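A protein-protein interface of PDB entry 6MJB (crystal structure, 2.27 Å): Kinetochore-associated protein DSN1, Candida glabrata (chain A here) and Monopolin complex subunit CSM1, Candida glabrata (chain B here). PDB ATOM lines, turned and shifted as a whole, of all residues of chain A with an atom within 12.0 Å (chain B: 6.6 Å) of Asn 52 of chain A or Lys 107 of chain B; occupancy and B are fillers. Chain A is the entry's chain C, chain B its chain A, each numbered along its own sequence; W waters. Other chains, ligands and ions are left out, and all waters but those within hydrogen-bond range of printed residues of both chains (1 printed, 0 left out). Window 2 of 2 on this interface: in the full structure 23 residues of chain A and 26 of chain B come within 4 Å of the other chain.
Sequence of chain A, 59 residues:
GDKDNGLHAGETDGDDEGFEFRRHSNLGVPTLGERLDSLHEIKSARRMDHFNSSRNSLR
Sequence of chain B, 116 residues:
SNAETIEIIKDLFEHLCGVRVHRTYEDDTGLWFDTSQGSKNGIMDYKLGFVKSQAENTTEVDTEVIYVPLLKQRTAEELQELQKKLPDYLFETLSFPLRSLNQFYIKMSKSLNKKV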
ATOM      1  N   MET A  48      17.379 -16.757  -2.842  1.00  0.00           N
ATOM      2  CA  MET A  48      18.599 -17.509  -2.571  1.00  0.00           C
ATOM      3  C   MET A  48      18.505 -18.057  -1.156  1.00  0.00           C
ATOM      4  O   MET A  48      18.073 -17.344  -0.249  1.00  0.00           O
ATOM      5  CB  MET A  48      19.845 -16.634  -2.682  1.00  0.00           C
ATOM      6  CG  MET A  48      20.422 -16.505  -4.055  1.00  0.00           C
ATOM      7  SD  MET A  48      22.097 -15.867  -3.888  1.00  0.00           S
ATOM      8  CE  MET A  48      22.995 -17.359  -3.481  1.00  0.00           C
ATOM      9  N   ASP A  49      18.933 -19.296  -0.948  1.00  0.00           N
ATOM     10  CA  ASP A  49      18.735 -19.884   0.375  1.00  0.00           C
ATOM     11  C   ASP A  49      19.881 -19.598   1.338  1.00  0.00           C
ATOM     12  O   ASP A  49      19.640 -19.339   2.522  1.00  0.00           O
ATOM     13  CB  ASP A  49      18.530 -21.399   0.269  1.00  0.00           C
ATOM     14  CG  ASP A  49      17.808 -21.968   1.482  1.00  0.00           C
ATOM     15  OD1 ASP A  49      16.585 -21.722   1.612  1.00  0.00           O
ATOM     16  OD2 ASP A  49      18.466 -22.631   2.314  1.00  0.00           O
ATOM     17  N   HIS A  50      21.119 -19.647   0.864  1.00  0.00           N
ATOM     18  CA  HIS A  50      22.283 -19.487   1.724  1.00  0.00           C
ATOM     19  C   HIS A  50      23.421 -18.894   0.903  1.00  0.00           C
ATOM     20  O   HIS A  50      23.277 -18.627  -0.290  1.00  0.00           O
ATOM     21  CB  HIS A  50      22.681 -20.828   2.342  1.00  0.00           C
ATOM     22  CG  HIS A  50      22.877 -21.904   1.329  1.00  0.00           C
ATOM     23  ND1 HIS A  50      21.823 -22.584   0.758  1.00  0.00           N
ATOM     24  CD2 HIS A  50      23.999 -22.387   0.745  1.00  0.00           C
ATOM     25  CE1 HIS A  50      22.291 -23.457  -0.117  1.00  0.00           C
ATOM     26  NE2 HIS A  50      23.607 -23.357  -0.145  1.00  0.00           N
ATOM     27  N   PHE A  51      24.570 -18.708   1.551  1.00  0.00           N
ATOM     28  CA  PHE A  51      25.727 -18.111   0.897  1.00  0.00           C
ATOM     29  C   PHE A  51      27.014 -18.870   1.214  1.00  0.00           C
ATOM     30  O   PHE A  51      28.098 -18.278   1.213  1.00  0.00           O
ATOM     31  CB  PHE A  51      25.875 -16.641   1.302  1.00  0.00           C
ATOM     32  CG  PHE A  51      24.709 -15.787   0.905  1.00  0.00           C
ATOM     33  CD1 PHE A  51      24.690 -15.147  -0.325  1.00  0.00           C
ATOM     34  CD2 PHE A  51      23.632 -15.611   1.765  1.00  0.00           C
ATOM     35  CE1 PHE A  51      23.619 -14.359  -0.702  1.00  0.00           C
ATOM     36  CE2 PHE A  51      22.549 -14.814   1.388  1.00  0.00           C
ATOM     37  CZ  PHE A  51      22.549 -14.194   0.154  1.00  0.00           C
ATOM     38  N   ASN A  52      26.916 -20.178   1.450  1.00  0.00           N
ATOM     39  CA  ASN A  52      28.025 -20.996   1.974  1.00  0.00           C
ATOM     40  C   ASN A  52      29.338 -20.894   1.186  1.00  0.00           C
ATOM     41  O   ASN A  52      29.365 -20.380   0.070  1.00  0.00           O
ATOM     42  CB  ASN A  52      27.592 -22.473   2.056  1.00  0.00           C
ATOM     43  CG  ASN A  52      27.218 -23.057   0.701  1.00  0.00           C
ATOM     44  OD1 ASN A  52      27.556 -22.498  -0.342  1.00  0.00           O
ATOM     45  ND2 ASN A  52      26.525 -24.199   0.710  1.00  0.00           N
ATOM     46  N   GLN B  37      28.602  -1.026   4.465  1.00  0.00           N
ATOM     47  CA  GLN B  37      29.514  -2.046   4.967  1.00  0.00           C
ATOM     48  C   GLN B  37      30.861  -1.931   4.271  1.00  0.00           C
ATOM     49  O   GLN B  37      30.928  -1.737   3.056  1.00  0.00           O
ATOM     50  CB  GLN B  37      28.943  -3.459   4.760  1.00  0.00           C
ATOM     51  CG  GLN B  37      29.807  -4.606   5.325  1.00  0.00           C
ATOM     52  CD  GLN B  37      29.195  -5.987   5.086  1.00  0.00           C
ATOM     53  OE1 GLN B  37      27.984  -6.131   4.983  1.00  0.00           O
ATOM     54  NE2 GLN B  37      30.041  -7.000   4.978  1.00  0.00           N
ATOM     55  N   LEU B  86      32.787  -8.410  -6.545  1.00  0.00           N
ATOM     56  CA  LEU B  86      31.488  -8.942  -6.134  1.00  0.00           C
ATOM     57  C   LEU B  86      31.005 -10.063  -7.046  1.00  0.00           C
ATOM     58  O   LEU B  86      31.046  -9.921  -8.278  1.00  0.00           O
ATOM     59  CB  LEU B  86      30.449  -7.825  -6.117  1.00  0.00           C
ATOM     60  CG  LEU B  86      30.692  -6.694  -5.119  1.00  0.00           C
ATOM     61  CD1 LEU B  86      29.500  -5.744  -5.126  1.00  0.00           C
ATOM     62  CD2 LEU B  86      30.965  -7.237  -3.716  1.00  0.00           C
ATOM     63  N   PRO B  87      30.517 -11.174  -6.481  1.00  0.00           N
ATOM     64  CA  PRO B  87      29.700 -12.118  -7.268  1.00  0.00           C
ATOM     65  C   PRO B  87      28.498 -11.420  -7.900  1.00  0.00           C
ATOM     66  O   PRO B  87      28.076 -10.379  -7.391  1.00  0.00           O
ATOM     67  CB  PRO B  87      29.235 -13.147  -6.227  1.00  0.00           C
ATOM     68  CG  PRO B  87      30.081 -12.934  -5.027  1.00  0.00           C
ATOM     69  CD  PRO B  87      30.585 -11.527  -5.056  1.00  0.00           C
ATOM     70  N   TYR B  89      25.293 -12.167  -7.856  1.00  0.00           N
ATOM     71  CA  TYR B  89      24.078 -12.078  -7.046  1.00  0.00           C
ATOM     72  C   TYR B  89      24.107 -10.894  -6.082  1.00  0.00           C
ATOM     73  O   TYR B  89      23.045 -10.411  -5.680  1.00  0.00           O
ATOM     74  CB  TYR B  89      23.824 -13.388  -6.287  1.00  0.00           C
ATOM     75  CG  TYR B  89      25.002 -13.935  -5.497  1.00  0.00           C
ATOM     76  CD1 TYR B  89      25.262 -13.491  -4.210  1.00  0.00           C
ATOM     77  CD2 TYR B  89      25.831 -14.923  -6.034  1.00  0.00           C
ATOM     78  CE1 TYR B  89      26.312 -13.990  -3.492  1.00  0.00           C
ATOM     79  CE2 TYR B  89      26.898 -15.440  -5.311  1.00  0.00           C
ATOM     80  CZ  TYR B  89      27.137 -14.963  -4.043  1.00  0.00           C
ATOM     81  OH  TYR B  89      28.192 -15.450  -3.309  1.00  0.00           O
ATOM     82  N   LEU B  90      25.296 -10.409  -5.703  1.00  0.00           N
ATOM     83  CA  LEU B  90      25.375  -9.227  -4.855  1.00  0.00           C
ATOM     84  C   LEU B  90      25.180  -7.938  -5.633  1.00  0.00           C
ATOM     85  O   LEU B  90      25.042  -6.877  -5.015  1.00  0.00           O
ATOM     86  CB  LEU B  90      26.705  -9.183  -4.097  1.00  0.00           C
ATOM     87  CG  LEU B  90      26.827 -10.234  -2.991  1.00  0.00           C
ATOM     88  CD1 LEU B  90      28.071 -10.032  -2.078  1.00  0.00           C
ATOM     89  CD2 LEU B  90      25.564 -10.289  -2.168  1.00  0.00           C
ATOM     90  N   ASN B 102      23.874 -13.675   8.582  1.00  0.00           N
ATOM     91  CA  ASN B 102      25.297 -13.657   8.909  1.00  0.00           C
ATOM     92  C   ASN B 102      26.139 -14.227   7.765  1.00  0.00           C
ATOM     93  O   ASN B 102      27.176 -13.654   7.399  1.00  0.00           O
ATOM     94  CB  ASN B 102      25.547 -14.422  10.212  1.00  0.00           C
ATOM     95  CG  ASN B 102      27.021 -14.457  10.592  1.00  0.00           C
ATOM     96  OD1 ASN B 102      27.595 -15.520  10.754  1.00  0.00           O
ATOM     97  ND2 ASN B 102      27.639 -13.286  10.698  1.00  0.00           N
ATOM     98  N   GLN B 103      25.705 -15.344   7.179  1.00  0.00           N
ATOM     99  CA  GLN B 103      26.372 -15.864   5.985  1.00  0.00           C
ATOM    100  C   GLN B 103      26.494 -14.798   4.907  1.00  0.00           C
ATOM    101  O   GLN B 103      27.556 -14.648   4.286  1.00  0.00           O
ATOM    102  CB  GLN B 103      25.609 -17.065   5.437  1.00  0.00           C
ATOM    103  CG  GLN B 103      25.740 -18.301   6.288  1.00  0.00           C
ATOM    104  CD  GLN B 103      24.943 -19.446   5.730  1.00  0.00           C
ATOM    105  OE1 GLN B 103      24.674 -19.503   4.523  1.00  0.00           O
ATOM    106  NE2 GLN B 103      24.551 -20.367   6.603  1.00  0.00           N
ATOM    107  N   PHE B 104      25.407 -14.043   4.682  1.00  0.00           N
ATOM    108  CA  PHE B 104      25.437 -12.925   3.741  1.00  0.00           C
ATOM    109  C   PHE B 104      26.507 -11.907   4.119  1.00  0.00           C
ATOM    110  O   PHE B 104      27.284 -11.466   3.262  1.00  0.00           O
ATOM    111  CB  PHE B 104      24.063 -12.242   3.673  1.00  0.00           C
ATOM    112  CG  PHE B 104      24.127 -10.810   3.205  1.00  0.00           C
ATOM    113  CD1 PHE B 104      24.085 -10.515   1.846  1.00  0.00           C
ATOM    114  CD2 PHE B 104      24.254  -9.763   4.126  1.00  0.00           C
ATOM    115  CE1 PHE B 104      24.132  -9.190   1.401  1.00  0.00           C
ATOM    116  CE2 PHE B 104      24.327  -8.438   3.698  1.00  0.00           C
ATOM    117  CZ  PHE B 104      24.256  -8.145   2.331  1.00  0.00           C
ATOM    118  N   TYR B 105      26.532 -11.488   5.396  1.00  0.00           N
ATOM    119  CA  TYR B 105      27.538 -10.521   5.844  1.00  0.00           C
ATOM    120  C   TYR B 105      28.946 -11.033   5.563  1.00  0.00           C
ATOM    121  O   TYR B 105      29.805 -10.291   5.071  1.00  0.00           O
ATOM    122  CB  TYR B 105      27.374 -10.202   7.340  1.00  0.00           C
ATOM    123  CG  TYR B 105      28.576  -9.475   7.914  1.00  0.00           C
ATOM    124  CD1 TYR B 105      28.607  -8.086   7.978  1.00  0.00           C
ATOM    125  CD2 TYR B 105      29.699 -10.183   8.382  1.00  0.00           C
ATOM    126  CE1 TYR B 105      29.720  -7.413   8.478  1.00  0.00           C
ATOM    127  CE2 TYR B 105      30.809  -9.524   8.875  1.00  0.00           C
ATOM    128  CZ  TYR B 105      30.815  -8.145   8.925  1.00  0.00           C
ATOM    129  OH  TYR B 105      31.913  -7.496   9.423  1.00  0.00           O
ATOM    130  N   ILE B 106      29.206 -12.306   5.884  1.00  0.00           N
ATOM    131  CA  ILE B 106      30.537 -12.881   5.661  1.00  0.00           C
ATOM    132  C   ILE B 106      30.867 -12.900   4.169  1.00  0.00           C
ATOM    133  O   ILE B 106      31.985 -12.566   3.755  1.00  0.00           O
ATOM    134  CB  ILE B 106      30.628 -14.287   6.285  1.00  0.00           C
ATOM    135  CG1 ILE B 106      30.553 -14.200   7.805  1.00  0.00           C
ATOM    136  CG2 ILE B 106      31.900 -15.019   5.849  1.00  0.00           C
ATOM    137  CD1 ILE B 106      30.521 -15.568   8.490  1.00  0.00           C
ATOM    138  N   LYS B 107      29.898 -13.289   3.335  1.00  0.00           N
ATOM    139  CA  LYS B 107      30.125 -13.225   1.894  1.00  0.00           C
ATOM    140  C   LYS B 107      30.481 -11.809   1.455  1.00  0.00           C
ATOM    141  O   LYS B 107      31.412 -11.616   0.663  1.00  0.00           O
ATOM    142  CB  LYS B 107      28.901 -13.732   1.128  1.00  0.00           C
ATOM    143  CG  LYS B 107      29.193 -14.897   0.201  1.00  0.00           C
ATOM    144  CD  LYS B 107      30.217 -14.541  -0.869  1.00  0.00           C
ATOM    145  CE  LYS B 107      31.066 -15.758  -1.261  1.00  0.00           C
ATOM    146  NZ  LYS B 107      30.400 -17.059  -0.995  1.00  0.00           N
ATOM    147  N   MET B 108      29.779 -10.804   1.986  1.00  0.00           N
ATOM    148  CA  MET B 108      30.027  -9.428   1.563  1.00  0.00           C
ATOM    149  C   MET B 108      31.369  -8.932   2.082  1.00  0.00           C
ATOM    150  O   MET B 108      32.105  -8.242   1.366  1.00  0.00           O
ATOM    151  CB  MET B 108      28.884  -8.514   2.030  1.00  0.00           C
ATOM    152  CG  MET B 108      29.073  -7.046   1.683  1.00  0.00           C
ATOM    153  SD  MET B 108      28.733  -6.661  -0.061  1.00  0.00           S
ATOM    154  CE  MET B 108      26.939  -6.922  -0.060  1.00  0.00           C
ATOM    155  N   SER B 109      31.697  -9.283   3.328  1.00  0.00           N
ATOM    156  CA  SER B 109      33.004  -8.961   3.893  1.00  0.00           C
ATOM    157  C   SER B 109      34.133  -9.524   3.039  1.00  0.00           C
ATOM    158  O   SER B 109      35.024  -8.786   2.604  1.00  0.00           O
ATOM    159  CB  SER B 109      33.091  -9.498   5.315  1.00  0.00           C
ATOM    160  OG  SER B 109      33.973  -8.706   6.082  1.00  0.00           O
ATOM    161  N   LYS B 110      34.100 -10.832   2.771  1.00  0.00           N
ATOM    162  CA  LYS B 110      35.153 -11.453   1.970  1.00  0.00           C
ATOM    163  C   LYS B 110      35.238 -10.834   0.581  1.00  0.00           C
ATOM    164  O   LYS B 110      36.341 -10.652   0.046  1.00  0.00           O
ATOM    165  CB  LYS B 110      34.916 -12.958   1.862  1.00  0.00           C
ATOM    166  CG  LYS B 110      35.059 -13.705   3.177  1.00  0.00           C
ATOM    167  CD  LYS B 110      34.863 -15.207   2.984  1.00  0.00           C
ATOM    168  CE  LYS B 110      35.109 -15.993   4.271  1.00  0.00           C
ATOM    169  NZ  LYS B 110      34.385 -17.304   4.255  1.00  0.00           N
ATOM    170  N   SER B 111      34.087 -10.512  -0.025  1.00  0.00           N
ATOM    171  CA  SER B 111      34.101  -9.912  -1.358  1.00  0.00           C
ATOM    172  C   SER B 111      34.725  -8.525  -1.324  1.00  0.00           C
ATOM    173  O   SER B 111      35.563  -8.188  -2.164  1.00  0.00           O
ATOM    174  CB  SER B 111      32.684  -9.843  -1.936  1.00  0.00           C
ATOM    175  OG  SER B 111      32.051 -11.109  -1.916  1.00  0.00           O
ATOM    176  N   LEU B 112      34.323  -7.698  -0.363  1.00  0.00           N
ATOM    177  CA  LEU B 112      34.903  -6.368  -0.278  1.00  0.00           C
ATOM    178  C   LEU B 112      36.393  -6.426   0.025  1.00  0.00           C
ATOM    179  O   LEU B 112      37.160  -5.604  -0.487  1.00  0.00           O
ATOM    180  CB  LEU B 112      34.176  -5.551   0.790  1.00  0.00           C
ATOM    181  CG  LEU B 112      32.719  -5.220   0.476  1.00  0.00           C
ATOM    182  CD1 LEU B 112      32.114  -4.463   1.634  1.00  0.00           C
ATOM    183  CD2 LEU B 112      32.629  -4.411  -0.801  1.00  0.00           C
HETATM  184  O   HOH W   1      29.124 -16.917   3.701  1.00  0.00           O
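OE1 of Gln 103 of chain B sits at hydrogen-bond distance from N of Phe 51 of chain A.
The backbone carbonyl oxygen (O) of Phe 51 of chain A lies within hydrogen-bond range of the side-chain amino group (NZ) of Lys 107 of chain B, at 3.4 Å.
OG of Ser 111 of chain B lies within hydrogen-bond range of O of Lys 107 of chain B (2.7 Å).
A ring nitrogen (NE2) of His 50 of chain A lies close to the side-chain amide nitrogen (ND2) of Asn 52 of chain A (3.2 Å).
Among the printed residues, merely in contact across the chains: His 50 of chain A with Gln 103 of chain B (3.2 Å), Asn 52 of chain A with Lys 107 of chain B (3.6 Å), Phe 51 of chain A with Tyr 89 of chain B (3.7 Å), Phe 51 of chain A with Phe 104 of chain B (3.8 Å), Met 48 of chain A with Tyr 89 of chain B (3.8 Å) and Asn 52 of chain A with Gln 103 of chain B (3.9 Å).
Of chain B, only Gln 103 and Lys 107 come within 4 Å of Asn 52 of chain A.
Of chain A, only Phe 51 and Asn 52 come within 4 Å of Lys 107 of chain B.
Of chain A, only His 50, Phe 51 and Asn 52 come within 4 Å of Gln 103 of chain B.
Phe 104 of chain B touches just one residue of chain A: Phe 51 (3.8 Å).
Met 108 of chain B touches none of the printed residues of chain A.
No residue of chain A comes within 4 Å of Ser 111 of chain B.
Of the printed residues of chain B, Met 48 of chain A touches Tyr 89.
Of the printed residues of chain A, Tyr 89 of chain B touches Met 48 and Phe 51.
Printed residues of chain B within 4 Å of Phe 51 of chain A: Tyr 89, Gln 103, Phe 104 and Lys 107.
Printed residues of chain B within 4 Å of His 50 of chain A: Gln 103 (3.2 Å).
The nearest printed residue of chain B that does not touch Met 48 of chain A is Leu 90 of chain B (6.6 Å).
Hydrophobic or aromatic side chains of chain A within 4 Å of the printed part of chain B: Met 48, His 50 and Phe 51.
Hydrophobic or aromatic side chains of chain B that line the printed part of chain A: Tyr 89 and Phe 104.
Water W1 lies within hydrogen-bond range of the backbone carbonyl oxygen (O) of Gln 103 of chain B (2.8 Å) and the backbone carbonyl oxygen (O) of Phe 51 of chain A (3.0 Å).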
